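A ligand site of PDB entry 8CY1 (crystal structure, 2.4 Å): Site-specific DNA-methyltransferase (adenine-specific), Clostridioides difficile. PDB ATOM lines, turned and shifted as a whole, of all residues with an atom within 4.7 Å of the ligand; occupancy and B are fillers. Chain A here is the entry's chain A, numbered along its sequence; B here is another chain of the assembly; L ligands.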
ATOM      1  N   GLY A  29       4.495  -2.608   5.120  1.00  0.00           N
ATOM      2  CA  GLY A  29       4.883  -1.284   5.565  1.00  0.00           C
ATOM      3  C   GLY A  29       6.258  -0.831   5.118  1.00  0.00           C
ATOM      4  O   GLY A  29       7.140  -0.574   5.946  1.00  0.00           O
ATOM      5  N   ILE A  30       6.456  -0.738   3.801  1.00  0.00           N
ATOM      6  CA  ILE A  30       7.693  -0.257   3.194  1.00  0.00           C
ATOM      7  C   ILE A  30       7.379   0.995   2.388  1.00  0.00           C
ATOM      8  O   ILE A  30       6.507   0.981   1.514  1.00  0.00           O
ATOM      9  CB  ILE A  30       8.346  -1.330   2.307  1.00  0.00           C
ATOM     10  N   TYR A  31       8.111   2.075   2.668  1.00  0.00           N
ATOM     11  CA  TYR A  31       7.882   3.387   2.062  1.00  0.00           C
ATOM     12  C   TYR A  31       9.070   3.787   1.194  1.00  0.00           C
ATOM     13  O   TYR A  31      10.224   3.526   1.558  1.00  0.00           O
ATOM     14  CB  TYR A  31       7.634   4.447   3.138  1.00  0.00           C
ATOM     15  CG  TYR A  31       6.489   4.122   4.069  1.00  0.00           C
ATOM     16  CD1 TYR A  31       6.680   3.344   5.203  1.00  0.00           C
ATOM     17  CD2 TYR A  31       5.210   4.612   3.824  1.00  0.00           C
ATOM     18  CE1 TYR A  31       5.629   3.046   6.061  1.00  0.00           C
ATOM     19  CE2 TYR A  31       4.159   4.321   4.666  1.00  0.00           C
ATOM     20  CZ  TYR A  31       4.368   3.538   5.785  1.00  0.00           C
ATOM     21  OH  TYR A  31       3.327   3.256   6.630  1.00  0.00           O
ATOM     22  N   ILE A  62      19.904   1.831   9.444  1.00  0.00           N
ATOM     23  CA  ILE A  62      19.198   0.892  10.304  1.00  0.00           C
ATOM     24  C   ILE A  62      17.750   0.692   9.874  1.00  0.00           C
ATOM     25  O   ILE A  62      16.996   0.019  10.575  1.00  0.00           O
ATOM     26  CB  ILE A  62      19.262   1.319  11.785  1.00  0.00           C
ATOM     27  CG1 ILE A  62      18.673   2.712  11.984  1.00  0.00           C
ATOM     28  CG2 ILE A  62      20.690   1.301  12.322  1.00  0.00           C
ATOM     29  CD1 ILE A  62      18.742   3.170  13.434  1.00  0.00           C
ATOM     30  N   SER A  63      17.347   1.260   8.730  1.00  0.00           N
ATOM     31  CA  SER A  63      16.014   1.054   8.154  1.00  0.00           C
ATOM     32  C   SER A  63      16.090   0.572   6.715  1.00  0.00           C
ATOM     33  O   SER A  63      15.062   0.551   6.033  1.00  0.00           O
ATOM     34  CB  SER A  63      15.215   2.351   8.230  1.00  0.00           C
ATOM     35  OG  SER A  63      14.644   2.552   9.500  1.00  0.00           O
ATOM     36  N   GLY A  65      15.685  -1.217   4.348  1.00  0.00           N
ATOM     37  CA  GLY A  65      14.615  -1.665   3.479  1.00  0.00           C
ATOM     38  C   GLY A  65      15.187  -2.437   2.305  1.00  0.00           C
ATOM     39  O   GLY A  65      15.987  -3.358   2.496  1.00  0.00           O
ATOM     40  N   ALA A 114      20.424  -2.671   8.197  1.00  0.00           N
ATOM     41  CA  ALA A 114      19.583  -3.441   9.092  1.00  0.00           C
ATOM     42  C   ALA A 114      18.125  -3.162   8.767  1.00  0.00           C
ATOM     43  O   ALA A 114      17.738  -2.016   8.553  1.00  0.00           O
ATOM     44  CB  ALA A 114      19.858  -3.100  10.559  1.00  0.00           C
ATOM     45  N   ASP A 115      17.326  -4.223   8.717  1.00  0.00           N
ATOM     46  CA  ASP A 115      15.885  -4.079   8.558  1.00  0.00           C
ATOM     47  C   ASP A 115      15.201  -5.293   9.144  1.00  0.00           C
ATOM     48  O   ASP A 115      15.742  -6.404   9.103  1.00  0.00           O
ATOM     49  CB  ASP A 115      15.484  -3.892   7.089  1.00  0.00           C
ATOM     50  CG  ASP A 115      14.088  -3.301   6.936  1.00  0.00           C
ATOM     51  OD1 ASP A 115      13.092  -3.976   7.291  1.00  0.00           O
ATOM     52  OD2 ASP A 115      13.988  -2.140   6.480  1.00  0.00           O
ATOM     53  N   ILE A 116      14.014  -5.077   9.710  1.00  0.00           N
ATOM     54  CA  ILE A 116      13.287  -6.152  10.352  1.00  0.00           C
ATOM     55  C   ILE A 116      12.626  -7.074   9.330  1.00  0.00           C
ATOM     56  O   ILE A 116      12.303  -8.224   9.667  1.00  0.00           O
ATOM     57  CB  ILE A 116      12.273  -5.555  11.338  1.00  0.00           C
ATOM     58  CG1 ILE A 116      11.815  -6.602  12.351  1.00  0.00           C
ATOM     59  CG2 ILE A 116      11.100  -4.906  10.592  1.00  0.00           C
ATOM     60  CD1 ILE A 116      11.141  -6.012  13.569  1.00  0.00           C
ATOM     61  N   ASP A 117      12.447  -6.624   8.089  1.00  0.00           N
ATOM     62  CA  ASP A 117      11.817  -7.409   7.038  1.00  0.00           C
ATOM     63  C   ASP A 117      12.892  -8.162   6.253  1.00  0.00           C
ATOM     64  O   ASP A 117      13.633  -7.560   5.477  1.00  0.00           O
ATOM     65  CB  ASP A 117      11.005  -6.498   6.111  1.00  0.00           C
ATOM     66  CG  ASP A 117      10.426  -7.232   4.916  1.00  0.00           C
ATOM     67  OD1 ASP A 117      10.188  -8.454   5.010  1.00  0.00           O
ATOM     68  OD2 ASP A 117      10.222  -6.588   3.863  1.00  0.00           O
ATOM     69  N   CYS A 149      16.907  -7.717  11.748  1.00  0.00           N
ATOM     70  CA  CYS A 149      16.748  -7.592  13.191  1.00  0.00           C
ATOM     71  C   CYS A 149      15.882  -6.374  13.506  1.00  0.00           C
ATOM     72  O   CYS A 149      15.596  -5.548  12.643  1.00  0.00           O
ATOM     73  CB  CYS A 149      18.109  -7.454  13.881  1.00  0.00           C
ATOM     74  SG  CYS A 149      18.902  -5.855  13.518  1.00  0.00           S
ATOM     75  N   ASP A 150      15.490  -6.292  14.768  1.00  0.00           N
ATOM     76  CA  ASP A 150      14.954  -5.055  15.338  1.00  0.00           C
ATOM     77  C   ASP A 150      16.139  -4.163  15.672  1.00  0.00           C
ATOM     78  O   ASP A 150      16.912  -4.464  16.593  1.00  0.00           O
ATOM     79  CB  ASP A 150      14.100  -5.361  16.564  1.00  0.00           C
ATOM     80  CG  ASP A 150      13.383  -4.130  17.107  1.00  0.00           C
ATOM     81  OD1 ASP A 150      13.825  -2.993  16.868  1.00  0.00           O
ATOM     82  OD2 ASP A 150      12.359  -4.326  17.801  1.00  0.00           O
ATOM     83  N   SER A 151      16.296  -3.055  14.937  1.00  0.00           N
ATOM     84  CA  SER A 151      17.430  -2.172  15.162  1.00  0.00           C
ATOM     85  C   SER A 151      17.414  -1.543  16.545  1.00  0.00           C
ATOM     86  O   SER A 151      18.472  -1.147  17.050  1.00  0.00           O
ATOM     87  CB  SER A 151      17.464  -1.082  14.095  1.00  0.00           C
ATOM     88  OG  SER A 151      17.660  -1.645  12.804  1.00  0.00           O
ATOM     89  N   LEU A 152      16.238  -1.449  17.176  1.00  0.00           N
ATOM     90  CA  LEU A 152      16.150  -0.905  18.524  1.00  0.00           C
ATOM     91  C   LEU A 152      16.556  -1.896  19.594  1.00  0.00           C
ATOM     92  O   LEU A 152      16.724  -1.506  20.746  1.00  0.00           O
ATOM     93  CB  LEU A 152      14.729  -0.410  18.785  1.00  0.00           C
ATOM     94  CG  LEU A 152      14.245   0.693  17.836  1.00  0.00           C
ATOM     95  CD1 LEU A 152      12.871   1.232  18.247  1.00  0.00           C
ATOM     96  CD2 LEU A 152      15.272   1.807  17.762  1.00  0.00           C
ATOM     97  N   ASN A 166      15.673   6.530   6.409  1.00  0.00           N
ATOM     98  CA  ASN A 166      14.285   6.954   6.650  1.00  0.00           C
ATOM     99  C   ASN A 166      13.650   5.979   7.637  1.00  0.00           C
ATOM    100  O   ASN A 166      13.222   4.880   7.236  1.00  0.00           O
ATOM    101  CB  ASN A 166      13.503   7.009   5.344  1.00  0.00           C
ATOM    102  CG  ASN A 166      12.063   7.459   5.541  1.00  0.00           C
ATOM    103  OD1 ASN A 166      11.687   7.971   6.588  1.00  0.00           O
ATOM    104  ND2 ASN A 166      11.244   7.277   4.504  1.00  0.00           N
ATOM    105  N   PRO A 167      13.569   6.342   8.918  1.00  0.00           N
ATOM    106  CA  PRO A 167      13.104   5.383   9.943  1.00  0.00           C
ATOM    107  C   PRO A 167      11.608   5.152   9.861  1.00  0.00           C
ATOM    108  O   PRO A 167      10.890   5.911   9.191  1.00  0.00           O
ATOM    109  CB  PRO A 167      13.483   6.085  11.263  1.00  0.00           C
ATOM    110  CG  PRO A 167      13.363   7.545  10.920  1.00  0.00           C
ATOM    111  CD  PRO A 167      13.851   7.671   9.482  1.00  0.00           C
ATOM    112  N   PRO A 168      11.098   4.115  10.513  1.00  0.00           N
ATOM    113  CA  PRO A 168       9.641   3.938  10.592  1.00  0.00           C
ATOM    114  C   PRO A 168       9.004   4.980  11.503  1.00  0.00           C
ATOM    115  O   PRO A 168       9.569   5.362  12.530  1.00  0.00           O
ATOM    116  CB  PRO A 168       9.481   2.528  11.175  1.00  0.00           C
ATOM    117  CG  PRO A 168      10.744   2.328  11.959  1.00  0.00           C
ATOM    118  CD  PRO A 168      11.815   2.994  11.149  1.00  0.00           C
ATOM    119  N   LEU A 175       0.955   1.706  17.613  1.00  0.00           N
ATOM    120  CA  LEU A 175       2.063   0.913  18.128  1.00  0.00           C
ATOM    121  C   LEU A 175       1.545  -0.137  19.103  1.00  0.00           C
ATOM    122  O   LEU A 175       0.697   0.163  19.946  1.00  0.00           O
ATOM    123  CB  LEU A 175       3.098   1.801  18.807  1.00  0.00           C
ATOM    124  CG  LEU A 175       4.432   1.137  19.131  1.00  0.00           C
ATOM    125  CD1 LEU A 175       4.970   0.403  17.911  1.00  0.00           C
ATOM    126  CD2 LEU A 175       5.438   2.166  19.608  1.00  0.00           C
ATOM    127  N   GLU A 176       2.040  -1.362  18.962  1.00  0.00           N
ATOM    128  CA  GLU A 176       1.580  -2.449  19.818  1.00  0.00           C
ATOM    129  C   GLU A 176       1.903  -2.166  21.277  1.00  0.00           C
ATOM    130  O   GLU A 176       2.981  -1.652  21.599  1.00  0.00           O
ATOM    131  CB  GLU A 176       2.211  -3.766  19.379  1.00  0.00           C
ATOM    132  CG  GLU A 176       1.420  -4.986  19.790  1.00  0.00           C
ATOM    133  CD  GLU A 176       2.300  -6.192  20.054  1.00  0.00           C
ATOM    134  OE1 GLU A 176       3.464  -5.988  20.439  1.00  0.00           O
ATOM    135  OE2 GLU A 176       1.820  -7.333  19.864  1.00  0.00           O
ATOM    136  N   TYR A 179       5.116  -3.871  22.668  1.00  0.00           N
ATOM    137  CA  TYR A 179       6.318  -3.168  22.236  1.00  0.00           C
ATOM    138  C   TYR A 179       6.461  -1.837  22.945  1.00  0.00           C
ATOM    139  O   TYR A 179       7.571  -1.453  23.342  1.00  0.00           O
ATOM    140  CB  TYR A 179       6.290  -2.968  20.722  1.00  0.00           C
ATOM    141  CG  TYR A 179       7.642  -2.678  20.135  1.00  0.00           C
ATOM    142  CD1 TYR A 179       8.487  -3.708  19.746  1.00  0.00           C
ATOM    143  CD2 TYR A 179       8.087  -1.369  19.990  1.00  0.00           C
ATOM    144  CE1 TYR A 179       9.726  -3.451  19.217  1.00  0.00           C
ATOM    145  CE2 TYR A 179       9.331  -1.095  19.462  1.00  0.00           C
ATOM    146  CZ  TYR A 179      10.146  -2.146  19.071  1.00  0.00           C
ATOM    147  OH  TYR A 179      11.388  -1.884  18.551  1.00  0.00           O
ATOM    148  N   LEU A 197       7.469   6.293  17.496  1.00  0.00           N
ATOM    149  CA  LEU A 197       8.539   5.318  17.344  1.00  0.00           C
ATOM    150  C   LEU A 197       9.805   5.928  16.762  1.00  0.00           C
ATOM    151  O   LEU A 197      10.914   5.541  17.141  1.00  0.00           O
ATOM    152  CB  LEU A 197       8.061   4.165  16.460  1.00  0.00           C
ATOM    153  CG  LEU A 197       9.102   3.078  16.178  1.00  0.00           C
ATOM    154  CD1 LEU A 197       9.416   2.302  17.448  1.00  0.00           C
ATOM    155  CD2 LEU A 197       8.599   2.143  15.095  1.00  0.00           C
ATOM    156  N   PHE A 201      14.505   5.992  17.097  1.00  0.00           N
ATOM    157  CA  PHE A 201      15.517   5.843  16.062  1.00  0.00           C
ATOM    158  C   PHE A 201      16.494   7.012  16.071  1.00  0.00           C
ATOM    159  O   PHE A 201      17.699   6.816  15.874  1.00  0.00           O
ATOM    160  CB  PHE A 201      14.850   5.680  14.694  1.00  0.00           C
ATOM    161  CG  PHE A 201      14.462   4.253  14.392  1.00  0.00           C
ATOM    162  CD1 PHE A 201      13.314   3.709  14.931  1.00  0.00           C
ATOM    163  CD2 PHE A 201      15.274   3.458  13.603  1.00  0.00           C
ATOM    164  CE1 PHE A 201      12.963   2.395  14.672  1.00  0.00           C
ATOM    165  CE2 PHE A 201      14.930   2.147  13.340  1.00  0.00           C
ATOM    166  CZ  PHE A 201      13.770   1.608  13.881  1.00  0.00           C
ATOM    167  P    DA B   8       0.012   9.090  11.875  1.00  0.00           P
ATOM    168  OP1  DA B   8      -1.082   8.136  11.580  1.00  0.00           O
ATOM    169  OP2  DA B   8       0.958   8.791  12.973  1.00  0.00           O
ATOM    170  O5'  DA B   8       0.832   9.352  10.542  1.00  0.00           O
ATOM    171  C5'  DA B   8       1.908   8.512  10.179  1.00  0.00           C
ATOM    172  C4'  DA B   8       2.038   8.472   8.673  1.00  0.00           C
ATOM    173  O4'  DA B   8       3.435   8.287   8.304  1.00  0.00           O
ATOM    174  C3'  DA B   8       1.273   7.349   7.983  1.00  0.00           C
ATOM    175  O3'  DA B   8       0.695   7.843   6.787  1.00  0.00           O
ATOM    176  C2'  DA B   8       2.362   6.326   7.683  1.00  0.00           C
ATOM    177  C1'  DA B   8       3.525   7.250   7.357  1.00  0.00           C
ATOM    178  N9   DA B   8       4.845   6.624   7.484  1.00  0.00           N
ATOM    179  C8   DA B   8       5.232   5.700   8.414  1.00  0.00           C
ATOM    180  N7   DA B   8       6.482   5.321   8.292  1.00  0.00           N
ATOM    181  C5   DA B   8       6.945   6.047   7.208  1.00  0.00           C
ATOM    182  C6   DA B   8       8.204   6.103   6.558  1.00  0.00           C
ATOM    183  N6   DA B   8       9.259   5.381   6.942  1.00  0.00           N
ATOM    184  N1   DA B   8       8.325   6.944   5.505  1.00  0.00           N
ATOM    185  C2   DA B   8       7.270   7.666   5.121  1.00  0.00           C
ATOM    186  N3   DA B   8       6.044   7.708   5.655  1.00  0.00           N
ATOM    187  C4   DA B   8       5.946   6.853   6.695  1.00  0.00           C
HETATM  188  C1  LIG L   1       3.896  -6.332  16.529  1.00  0.00           C
HETATM  189  C2  LIG L   1       4.834  -6.076  17.506  1.00  0.00           C
HETATM  190  C3  LIG L   1       5.647  -4.963  17.414  1.00  0.00           C
HETATM  191  C4  LIG L   1       5.535  -4.087  16.340  1.00  0.00           C
HETATM  192  C5  LIG L   1       6.446  -2.890  16.224  1.00  0.00           C
HETATM  193  C6  LIG L   1       7.771  -3.200  15.543  1.00  0.00           C
HETATM  194  C7  LIG L   1       8.780  -2.069  15.635  1.00  0.00           C
HETATM  195  C8  LIG L   1      10.165  -2.470  15.165  1.00  0.00           C
HETATM  196  C9  LIG L   1      11.158  -1.332  15.198  1.00  0.00           C
HETATM  197  C10 LIG L   1      12.871  -1.848  13.459  1.00  0.00           C
HETATM  198  N1  LIG L   1      13.891  -2.024  10.834  1.00  0.00           N
HETATM  199  C11 LIG L   1      14.561  -2.289  11.963  1.00  0.00           C
HETATM  200  C12 LIG L   1      12.633  -1.655  11.097  1.00  0.00           C
HETATM  201  N2  LIG L   1      10.717  -1.160  12.233  1.00  0.00           N
HETATM  202  C13 LIG L   1      10.596  -1.517   7.937  1.00  0.00           C
HETATM  203  C14 LIG L   1      10.539  -1.029  10.933  1.00  0.00           C
HETATM  204  C15 LIG L   1      12.047  -1.557  12.347  1.00  0.00           C
HETATM  205  C16 LIG L   1      11.822  -1.142   8.756  1.00  0.00           C
HETATM  206  C17 LIG L   1      10.575   1.819   7.453  1.00  0.00           C
HETATM  207  O1  LIG L   1      12.065   0.232   8.501  1.00  0.00           O
HETATM  208  C18 LIG L   1      11.471   0.618   7.240  1.00  0.00           C
HETATM  209  O2  LIG L   1       9.220   1.504   7.165  1.00  0.00           O
HETATM  210  N3  LIG L   1      11.655  -1.299  10.195  1.00  0.00           N
HETATM  211  C19 LIG L   1      10.762  -0.620   6.692  1.00  0.00           C
HETATM  212  O3  LIG L   1      11.527  -1.249   5.669  1.00  0.00           O
HETATM  213  C20 LIG L   1       3.772  -5.476  15.459  1.00  0.00           C
HETATM  214  C21 LIG L   1       4.584  -4.363  15.366  1.00  0.00           C
HETATM  215  N4  LIG L   1      14.139  -2.228  13.223  1.00  0.00           N
HETATM  216  N5  LIG L   1      12.471  -1.752  14.740  1.00  0.00           N
HETATM  217  O4  LIG L   1      10.677  -2.890   7.594  1.00  0.00           O
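OD1 of Asp 150 sits at hydrogen-bond distance from N5 of the ligand, at 2.8 Å. A nitrogen (N4) of the ligand is in hydrogen-bond range of the backbone NH (N) of Ser 151, 2.9 Å away. An oxygen (O4) of the ligand lies within hydrogen-bond range of the side-chain carboxylate (OD1) of Asp 115 (2.7 Å). A nitrogen (N1) of the ligand is in hydrogen-bond range of the backbone NH (N) of Ile 116 (3.3 Å). The backbone carbonyl oxygen (O) of Gly 29 is in hydrogen-bond range of an oxygen (O2) of the ligand, 3.2 Å away.
The side-chain carboxylate of Glu 176 lies within hydrogen-bond range of the backbone NH of Tyr 179, 3.5 Å away. N1 of DA 8 of chain B is in hydrogen-bond range of the side-chain amide nitrogen (ND2) of Asn 166 (3.1 Å). The backbone carbonyl oxygen (O) of Asp 115 is in hydrogen-bond range of the backbone NH (N) of Cys 149, at 3.2 Å. OD2 of Asp 115 is in hydrogen-bond range of N of Gly 65. The backbone NH (N) of Ser 63 sits at hydrogen-bond distance from the backbone carbonyl oxygen (O) of Ala 114, at 3.3 Å. The backbone NH (N) of Ile 116 lies close to the backbone carbonyl oxygen (O) of Cys 149, at 3.4 Å. The side-chain carboxylate (OD1) of Asp 115 lies within hydrogen-bond range of the backbone NH (N) of Asp 117 (2.8 Å). OH of Tyr 179 lies within hydrogen-bond range of OD2 of Asp 150, at 2.7 Å.
Merely in contact with the ligand: Glu 176 (3.2 Å), Tyr 179 (3.4 Å), Cys 149 (3.5 Å), Pro 168 (3.5 Å), Phe 201 (3.6 Å), Ser 63 (3.6 Å), Ile 62 (3.6 Å), Tyr 31 (3.7 Å), Gly 65 (3.8 Å), DA 8 of chain B (3.8 Å), Asp 117 (3.9 Å) and Leu 175 (3.98 Å). Hydrophobic or aromatic side chains within 4 Å of the ligand: Tyr 31, Ile 116, Pro 168, Leu 175, Tyr 179 and Phe 201. Of the 23 residues printed, 17 come within 4 Å of the ligand. Along chain A the residues within 4 Å of the ligand span positions 29 to 201.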
